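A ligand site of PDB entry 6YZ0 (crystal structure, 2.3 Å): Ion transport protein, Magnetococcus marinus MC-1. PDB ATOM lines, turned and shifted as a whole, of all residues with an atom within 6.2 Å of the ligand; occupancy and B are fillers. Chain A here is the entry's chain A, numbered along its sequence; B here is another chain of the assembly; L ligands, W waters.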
ATOM      1  N   ARG A 189      13.074 -23.298 -28.945  1.00  0.00           N
ATOM      2  CA  ARG A 189      11.636 -23.710 -28.879  1.00  0.00           C
ATOM      3  C   ARG A 189      11.540 -25.179 -28.366  1.00  0.00           C
ATOM      4  O   ARG A 189      10.795 -25.393 -27.413  1.00  0.00           O
ATOM      5  CB  ARG A 189      10.859 -23.509 -30.145  1.00  0.00           C
ATOM      6  CG  ARG A 189      10.704 -22.079 -30.554  1.00  0.00           C
ATOM      7  CD  ARG A 189       9.848 -22.090 -31.792  1.00  0.00           C
ATOM      8  NE  ARG A 189       9.717 -20.779 -32.399  1.00  0.00           N
ATOM      9  CZ  ARG A 189       8.846 -19.857 -31.987  1.00  0.00           C
ATOM     10  NH1 ARG A 189       8.055 -20.084 -30.941  1.00  0.00           N
ATOM     11  NH2 ARG A 189       8.745 -18.705 -32.630  1.00  0.00           N
ATOM     12  N   MET A 192      12.026 -24.857 -24.569  1.00  0.00           N
ATOM     13  CA  MET A 192      10.923 -24.199 -23.874  1.00  0.00           C
ATOM     14  C   MET A 192       9.709 -25.090 -23.719  1.00  0.00           C
ATOM     15  O   MET A 192       8.876 -24.791 -22.873  1.00  0.00           O
ATOM     16  CB  MET A 192      10.525 -22.851 -24.476  1.00  0.00           C
ATOM     17  CG  MET A 192      11.581 -21.763 -24.326  1.00  0.00           C
ATOM     18  SD  MET A 192      10.899 -20.177 -24.910  1.00  0.00           S
ATOM     19  CE  MET A 192      10.592 -20.568 -26.677  1.00  0.00           C
ATOM     20  N   HIS A 195      11.113 -26.465 -20.360  1.00  0.00           N
ATOM     21  CA  HIS A 195      11.469 -25.380 -19.453  1.00  0.00           C
ATOM     22  C   HIS A 195      10.934 -24.064 -20.059  1.00  0.00           C
ATOM     23  O   HIS A 195      11.663 -23.395 -20.774  1.00  0.00           O
ATOM     24  CB  HIS A 195      12.995 -25.310 -19.323  1.00  0.00           C
ATOM     25  CG  HIS A 195      13.669 -26.631 -19.064  1.00  0.00           C
ATOM     26  ND1 HIS A 195      13.825 -27.117 -17.777  1.00  0.00           N
ATOM     27  CD2 HIS A 195      14.191 -27.526 -19.927  1.00  0.00           C
ATOM     28  CE1 HIS A 195      14.455 -28.275 -17.904  1.00  0.00           C
ATOM     29  NE2 HIS A 195      14.681 -28.564 -19.181  1.00  0.00           N
ATOM     30  N   PRO A 196       9.673 -23.670 -19.752  1.00  0.00           N
ATOM     31  CA  PRO A 196       9.095 -22.476 -20.408  1.00  0.00           C
ATOM     32  C   PRO A 196       9.842 -21.124 -20.234  1.00  0.00           C
ATOM     33  O   PRO A 196       9.653 -20.223 -21.052  1.00  0.00           O
ATOM     34  CB  PRO A 196       7.664 -22.374 -19.821  1.00  0.00           C
ATOM     35  CG  PRO A 196       7.545 -23.450 -18.788  1.00  0.00           C
ATOM     36  CD  PRO A 196       8.674 -24.401 -18.927  1.00  0.00           C
ATOM     37  N   ASN A 197      10.655 -20.975 -19.214  1.00  0.00           N
ATOM     38  CA  ASN A 197      11.399 -19.743 -18.986  1.00  0.00           C
ATOM     39  C   ASN A 197      12.790 -19.748 -19.596  1.00  0.00           C
ATOM     40  O   ASN A 197      13.527 -18.795 -19.386  1.00  0.00           O
ATOM     41  CB  ASN A 197      11.498 -19.463 -17.489  1.00  0.00           C
ATOM     42  CG  ASN A 197      10.154 -19.156 -16.882  1.00  0.00           C
ATOM     43  OD1 ASN A 197       9.377 -18.343 -17.418  1.00  0.00           O
ATOM     44  ND2 ASN A 197       9.839 -19.795 -15.767  1.00  0.00           N
ATOM     45  N   ALA A 198      13.170 -20.785 -20.370  1.00  0.00           N
ATOM     46  CA  ALA A 198      14.502 -20.861 -20.958  1.00  0.00           C
ATOM     47  C   ALA A 198      14.881 -19.631 -21.794  1.00  0.00           C
ATOM     48  O   ALA A 198      16.047 -19.384 -21.950  1.00  0.00           O
ATOM     49  CB  ALA A 198      14.667 -22.128 -21.765  1.00  0.00           C
ATOM     50  N   TRP A 199      13.898 -18.877 -22.336  1.00  0.00           N
ATOM     51  CA  TRP A 199      14.191 -17.690 -23.134  1.00  0.00           C
ATOM     52  C   TRP A 199      14.928 -16.639 -22.297  1.00  0.00           C
ATOM     53  O   TRP A 199      15.706 -15.883 -22.843  1.00  0.00           O
ATOM     54  CB  TRP A 199      12.911 -17.100 -23.744  1.00  0.00           C
ATOM     55  CG  TRP A 199      11.914 -16.674 -22.724  1.00  0.00           C
ATOM     56  CD1 TRP A 199      10.929 -17.442 -22.171  1.00  0.00           C
ATOM     57  CD2 TRP A 199      11.842 -15.395 -22.078  1.00  0.00           C
ATOM     58  NE1 TRP A 199      10.233 -16.714 -21.239  1.00  0.00           N
ATOM     59  CE2 TRP A 199      10.779 -15.455 -21.150  1.00  0.00           C
ATOM     60  CE3 TRP A 199      12.587 -14.213 -22.169  1.00  0.00           C
ATOM     61  CZ2 TRP A 199      10.439 -14.373 -20.346  1.00  0.00           C
ATOM     62  CZ3 TRP A 199      12.242 -13.140 -21.366  1.00  0.00           C
ATOM     63  CH2 TRP A 199      11.167 -13.225 -20.471  1.00  0.00           C
ATOM     64  N   ILE A 203      18.025 -15.655 -24.631  1.00  0.00           N
ATOM     65  CA  ILE A 203      17.931 -14.361 -25.330  1.00  0.00           C
ATOM     66  C   ILE A 203      19.040 -13.392 -24.810  1.00  0.00           C
ATOM     67  O   ILE A 203      19.858 -12.949 -25.633  1.00  0.00           O
ATOM     68  CB  ILE A 203      16.499 -13.777 -25.333  1.00  0.00           C
ATOM     69  CG1 ILE A 203      15.600 -14.648 -26.257  1.00  0.00           C
ATOM     70  CG2 ILE A 203      16.512 -12.298 -25.750  1.00  0.00           C
ATOM     71  CD1 ILE A 203      14.162 -14.206 -26.379  1.00  0.00           C
ATOM     72  N   MET A 207      22.180 -11.724 -26.978  1.00  0.00           N
ATOM     73  CA  MET A 207      22.398 -10.284 -27.010  1.00  0.00           C
ATOM     74  C   MET A 207      23.828  -9.924 -26.600  1.00  0.00           C
ATOM     75  O   MET A 207      24.534  -9.261 -27.355  1.00  0.00           O
ATOM     76  CB  MET A 207      21.369  -9.542 -26.148  1.00  0.00           C
ATOM     77  CG  MET A 207      19.934  -9.690 -26.654  1.00  0.00           C
ATOM     78  SD  MET A 207      18.764  -9.040 -25.416  1.00  0.00           S
ATOM     79  CE  MET A 207      17.294  -8.666 -26.467  1.00  0.00           C
ATOM     80  N   PHE B 145       9.330  -2.962 -31.660  1.00  0.00           N
ATOM     81  CA  PHE B 145       9.040  -4.304 -31.216  1.00  0.00           C
ATOM     82  C   PHE B 145       7.654  -4.409 -30.606  1.00  0.00           C
ATOM     83  O   PHE B 145       6.901  -5.306 -30.963  1.00  0.00           O
ATOM     84  CB  PHE B 145      10.092  -4.767 -30.207  1.00  0.00           C
ATOM     85  CG  PHE B 145      10.991  -5.799 -30.839  1.00  0.00           C
ATOM     86  CD1 PHE B 145      12.123  -5.409 -31.527  1.00  0.00           C
ATOM     87  CD2 PHE B 145      10.647  -7.133 -30.833  1.00  0.00           C
ATOM     88  CE1 PHE B 145      12.912  -6.347 -32.154  1.00  0.00           C
ATOM     89  CE2 PHE B 145      11.445  -8.067 -31.447  1.00  0.00           C
ATOM     90  CZ  PHE B 145      12.564  -7.682 -32.117  1.00  0.00           C
ATOM     91  N   GLU B 162       0.687 -20.869 -31.821  1.00  0.00           N
ATOM     92  CA  GLU B 162       1.988 -21.248 -31.208  1.00  0.00           C
ATOM     93  C   GLU B 162       2.999 -20.113 -31.315  1.00  0.00           C
ATOM     94  O   GLU B 162       3.752 -19.872 -30.390  1.00  0.00           O
ATOM     95  CB  GLU B 162       2.546 -22.538 -31.843  1.00  0.00           C
ATOM     96  CG  GLU B 162       3.921 -22.888 -31.282  1.00  0.00           C
ATOM     97  CD  GLU B 162       4.644 -24.057 -31.927  1.00  0.00           C
ATOM     98  OE1 GLU B 162       4.112 -24.622 -32.912  1.00  0.00           O
ATOM     99  OE2 GLU B 162       5.785 -24.345 -31.493  1.00  0.00           O
ATOM    100  N   ASP B 166      -0.334 -14.866 -28.240  1.00  0.00           N
ATOM    101  CA  ASP B 166      -0.348 -13.854 -27.195  1.00  0.00           C
ATOM    102  C   ASP B 166       0.832 -12.878 -27.401  1.00  0.00           C
ATOM    103  O   ASP B 166       1.748 -13.152 -28.175  1.00  0.00           O
ATOM    104  CB  ASP B 166      -0.427 -14.474 -25.780  1.00  0.00           C
ATOM    105  CG  ASP B 166       0.811 -15.172 -25.277  1.00  0.00           C
ATOM    106  OD1 ASP B 166       1.908 -14.760 -25.644  1.00  0.00           O
ATOM    107  OD2 ASP B 166       0.671 -16.123 -24.494  1.00  0.00           O
ATOM    108  N   SER B 168       3.458 -12.089 -25.496  1.00  0.00           N
ATOM    109  CA  SER B 168       4.725 -12.700 -25.139  1.00  0.00           C
ATOM    110  C   SER B 168       5.237 -13.618 -26.264  1.00  0.00           C
ATOM    111  O   SER B 168       6.411 -13.598 -26.627  1.00  0.00           O
ATOM    112  CB  SER B 168       4.544 -13.529 -23.870  1.00  0.00           C
ATOM    113  OG  SER B 168       4.566 -12.651 -22.764  1.00  0.00           O
ATOM    114  N   LYS B 169       4.340 -14.421 -26.828  1.00  0.00           N
ATOM    115  CA  LYS B 169       4.653 -15.324 -27.904  1.00  0.00           C
ATOM    116  C   LYS B 169       5.024 -14.536 -29.111  1.00  0.00           C
ATOM    117  O   LYS B 169       5.993 -14.901 -29.727  1.00  0.00           O
ATOM    118  CB  LYS B 169       3.472 -16.249 -28.232  1.00  0.00           C
ATOM    119  CG  LYS B 169       3.234 -17.344 -27.221  1.00  0.00           C
ATOM    120  CD  LYS B 169       2.009 -18.171 -27.715  1.00  0.00           C
ATOM    121  CE  LYS B 169       1.752 -19.404 -26.917  1.00  0.00           C
ATOM    122  NZ  LYS B 169       0.568 -20.134 -27.467  1.00  0.00           N
ATOM    123  N   SER B 170       4.308 -13.445 -29.433  1.00  0.00           N
ATOM    124  CA  SER B 170       4.678 -12.613 -30.583  1.00  0.00           C
ATOM    125  C   SER B 170       6.015 -11.931 -30.388  1.00  0.00           C
ATOM    126  O   SER B 170       6.776 -11.846 -31.334  1.00  0.00           O
ATOM    127  CB  SER B 170       3.627 -11.562 -30.867  1.00  0.00           C
ATOM    128  OG  SER B 170       2.432 -12.231 -31.193  1.00  0.00           O
ATOM    129  N   LEU B 171       6.314 -11.449 -29.165  1.00  0.00           N
ATOM    130  CA  LEU B 171       7.609 -10.791 -28.918  1.00  0.00           C
ATOM    131  C   LEU B 171       8.763 -11.772 -29.195  1.00  0.00           C
ATOM    132  O   LEU B 171       9.746 -11.421 -29.848  1.00  0.00           O
ATOM    133  CB  LEU B 171       7.704 -10.242 -27.494  1.00  0.00           C
ATOM    134  CG  LEU B 171       6.875  -8.969 -27.216  1.00  0.00           C
ATOM    135  CD1 LEU B 171       6.612  -8.781 -25.695  1.00  0.00           C
ATOM    136  CD2 LEU B 171       7.544  -7.713 -27.820  1.00  0.00           C
ATOM    137  N   TYR B 172       8.599 -13.015 -28.740  1.00  0.00           N
ATOM    138  CA  TYR B 172       9.587 -14.051 -28.942  1.00  0.00           C
ATOM    139  C   TYR B 172       9.825 -14.367 -30.428  1.00  0.00           C
ATOM    140  O   TYR B 172      10.974 -14.482 -30.842  1.00  0.00           O
ATOM    141  CB  TYR B 172       9.218 -15.343 -28.156  1.00  0.00           C
ATOM    142  CG  TYR B 172      10.226 -16.460 -28.379  1.00  0.00           C
ATOM    143  CD1 TYR B 172      10.122 -17.312 -29.468  1.00  0.00           C
ATOM    144  CD2 TYR B 172      11.303 -16.632 -27.522  1.00  0.00           C
ATOM    145  CE1 TYR B 172      11.091 -18.259 -29.749  1.00  0.00           C
ATOM    146  CE2 TYR B 172      12.245 -17.637 -27.749  1.00  0.00           C
ATOM    147  CZ  TYR B 172      12.149 -18.419 -28.891  1.00  0.00           C
ATOM    148  OH  TYR B 172      13.020 -19.423 -29.157  1.00  0.00           O
ATOM    149  N   THR B 173       8.747 -14.565 -31.229  1.00  0.00           N
ATOM    150  CA  THR B 173       8.946 -14.934 -32.634  1.00  0.00           C
ATOM    151  C   THR B 173       9.393 -13.725 -33.450  1.00  0.00           C
ATOM    152  O   THR B 173      10.129 -13.932 -34.395  1.00  0.00           O
ATOM    153  CB  THR B 173       7.818 -15.775 -33.283  1.00  0.00           C
ATOM    154  OG1 THR B 173       7.147 -15.145 -34.355  1.00  0.00           O
ATOM    155  CG2 THR B 173       6.855 -16.301 -32.339  1.00  0.00           C
ATOM    156  N   PHE B 175      11.606 -11.533 -32.272  1.00  0.00           N
ATOM    157  CA  PHE B 175      13.029 -11.494 -31.959  1.00  0.00           C
ATOM    158  C   PHE B 175      13.730 -12.548 -32.841  1.00  0.00           C
ATOM    159  O   PHE B 175      14.810 -12.257 -33.357  1.00  0.00           O
ATOM    160  CB  PHE B 175      13.295 -11.792 -30.465  1.00  0.00           C
ATOM    161  CG  PHE B 175      14.775 -11.826 -30.127  1.00  0.00           C
ATOM    162  CD1 PHE B 175      15.480 -10.663 -29.914  1.00  0.00           C
ATOM    163  CD2 PHE B 175      15.483 -13.028 -30.160  1.00  0.00           C
ATOM    164  CE1 PHE B 175      16.852 -10.681 -29.677  1.00  0.00           C
ATOM    165  CE2 PHE B 175      16.859 -13.048 -29.932  1.00  0.00           C
ATOM    166  CZ  PHE B 175      17.534 -11.868 -29.690  1.00  0.00           C
ATOM    167  N   MET B 178      13.791 -11.141 -36.328  1.00  0.00           N
ATOM    168  CA  MET B 178      14.820 -10.091 -36.402  1.00  0.00           C
ATOM    169  C   MET B 178      16.235 -10.714 -36.518  1.00  0.00           C
ATOM    170  O   MET B 178      17.096 -10.189 -37.219  1.00  0.00           O
ATOM    171  CB  MET B 178      14.743  -9.145 -35.195  1.00  0.00           C
ATOM    172  CG  MET B 178      15.889  -8.092 -35.188  1.00  0.00           C
ATOM    173  SD  MET B 178      15.910  -7.149 -33.647  1.00  0.00           S
ATOM    174  CE  MET B 178      16.511  -8.342 -32.533  1.00  0.00           C
HETATM  175  C1  LIG L   1      12.292 -10.031 -26.194  1.00  0.00           C
HETATM  176  C2  LIG L   1      11.258 -11.148 -26.296  1.00  0.00           C
HETATM  177  C3  LIG L   1      11.020 -11.918 -25.018  1.00  0.00           C
HETATM  178  C4  LIG L   1       9.822 -12.829 -25.070  1.00  0.00           C
HETATM  179  C5  LIG L   1       9.396 -13.332 -23.718  1.00  0.00           C
HETATM  180  C6  LIG L   1       8.176 -14.233 -23.716  1.00  0.00           C
HETATM  181  C7  LIG L   1       8.459 -15.672 -24.139  1.00  0.00           C
HETATM  182  C8  LIG L   1       7.410 -16.646 -23.629  1.00  0.00           C
HETATM  183  N1  LIG L   1       7.201 -17.779 -24.327  1.00  0.00           N
HETATM  184  O1  LIG L   1       6.810 -16.401 -22.593  1.00  0.00           O
HETATM  185  C9  LIG L   1       7.935 -18.131 -25.553  1.00  0.00           C
HETATM  186  C10 LIG L   1       6.189 -18.748 -23.879  1.00  0.00           C
HETATM  187  C11 LIG L   1       6.657 -20.168 -23.554  1.00  0.00           C
HETATM  188  C12 LIG L   1       5.651 -20.922 -22.695  1.00  0.00           C
HETATM  189  O2  LIG L   1       7.908 -20.154 -22.869  1.00  0.00           O
HETATM  190  O3  LIG L   1       4.396 -21.053 -23.371  1.00  0.00           O
HETATM  191  C13 LIG L   1       7.056 -18.223 -26.774  1.00  0.00           C
HETATM  192  O4  LIG L   1       6.740 -19.565 -27.083  1.00  0.00           O
HETATM  193  C14 LIG L   1      12.500  -9.276 -27.482  1.00  0.00           C
HETATM  194  C15 LIG L   1      13.542  -8.186 -27.404  1.00  0.00           C
HETATM  195  O   HOH W   1       4.569 -21.093 -28.321  1.00  0.00           O
HETATM  196  O   HOH W   2       6.377 -17.919 -29.680  1.00  0.00           O
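Water W1 bridges O of Glu 162 of chain B and O4 of the ligand. Water W2 lies within hydrogen-bond range of NH1 of Arg 189 (3.0 Å), O of Lys 169 of chain B (3.0 Å), O4 of the ligand (3.1 Å) and O of Glu 162 of chain B (3.3 Å).
Trp 199 touches the ligand (NE1 to C7, 3.6 Å). CE of Met 207 touches C15 of the ligand, at 3.9 Å. O of Ser 168 of chain B touches C6 of the ligand (3.5 Å). CA of Lys 169 of chain B touches C13 of the ligand, 3.9 Å away. CB of Leu 171 of chain B touches C2 of the ligand (3.9 Å). CB of Tyr 172 of chain B touches C13 of the ligand (3.9 Å). CB of Phe 175 of chain B touches C14 of the ligand (3.98 Å). Hydrophobic or aromatic side chains within 4 Å of the ligand: Met 192, Pro 196, Trp 199, Met 207, Leu 171 of chain B, Tyr 172 of chain B and Phe 175 of chain B. Of the 20 residues printed, 9 come within 4 Å of the ligand.
An oxygen (O2) of the ligand sits at hydrogen-bond distance from the backbone carbonyl oxygen (O) of Pro 196 (2.5 Å). An oxygen (O2) of the ligand lies within hydrogen-bond range of the side-chain sulfur (SD) of Met 192.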
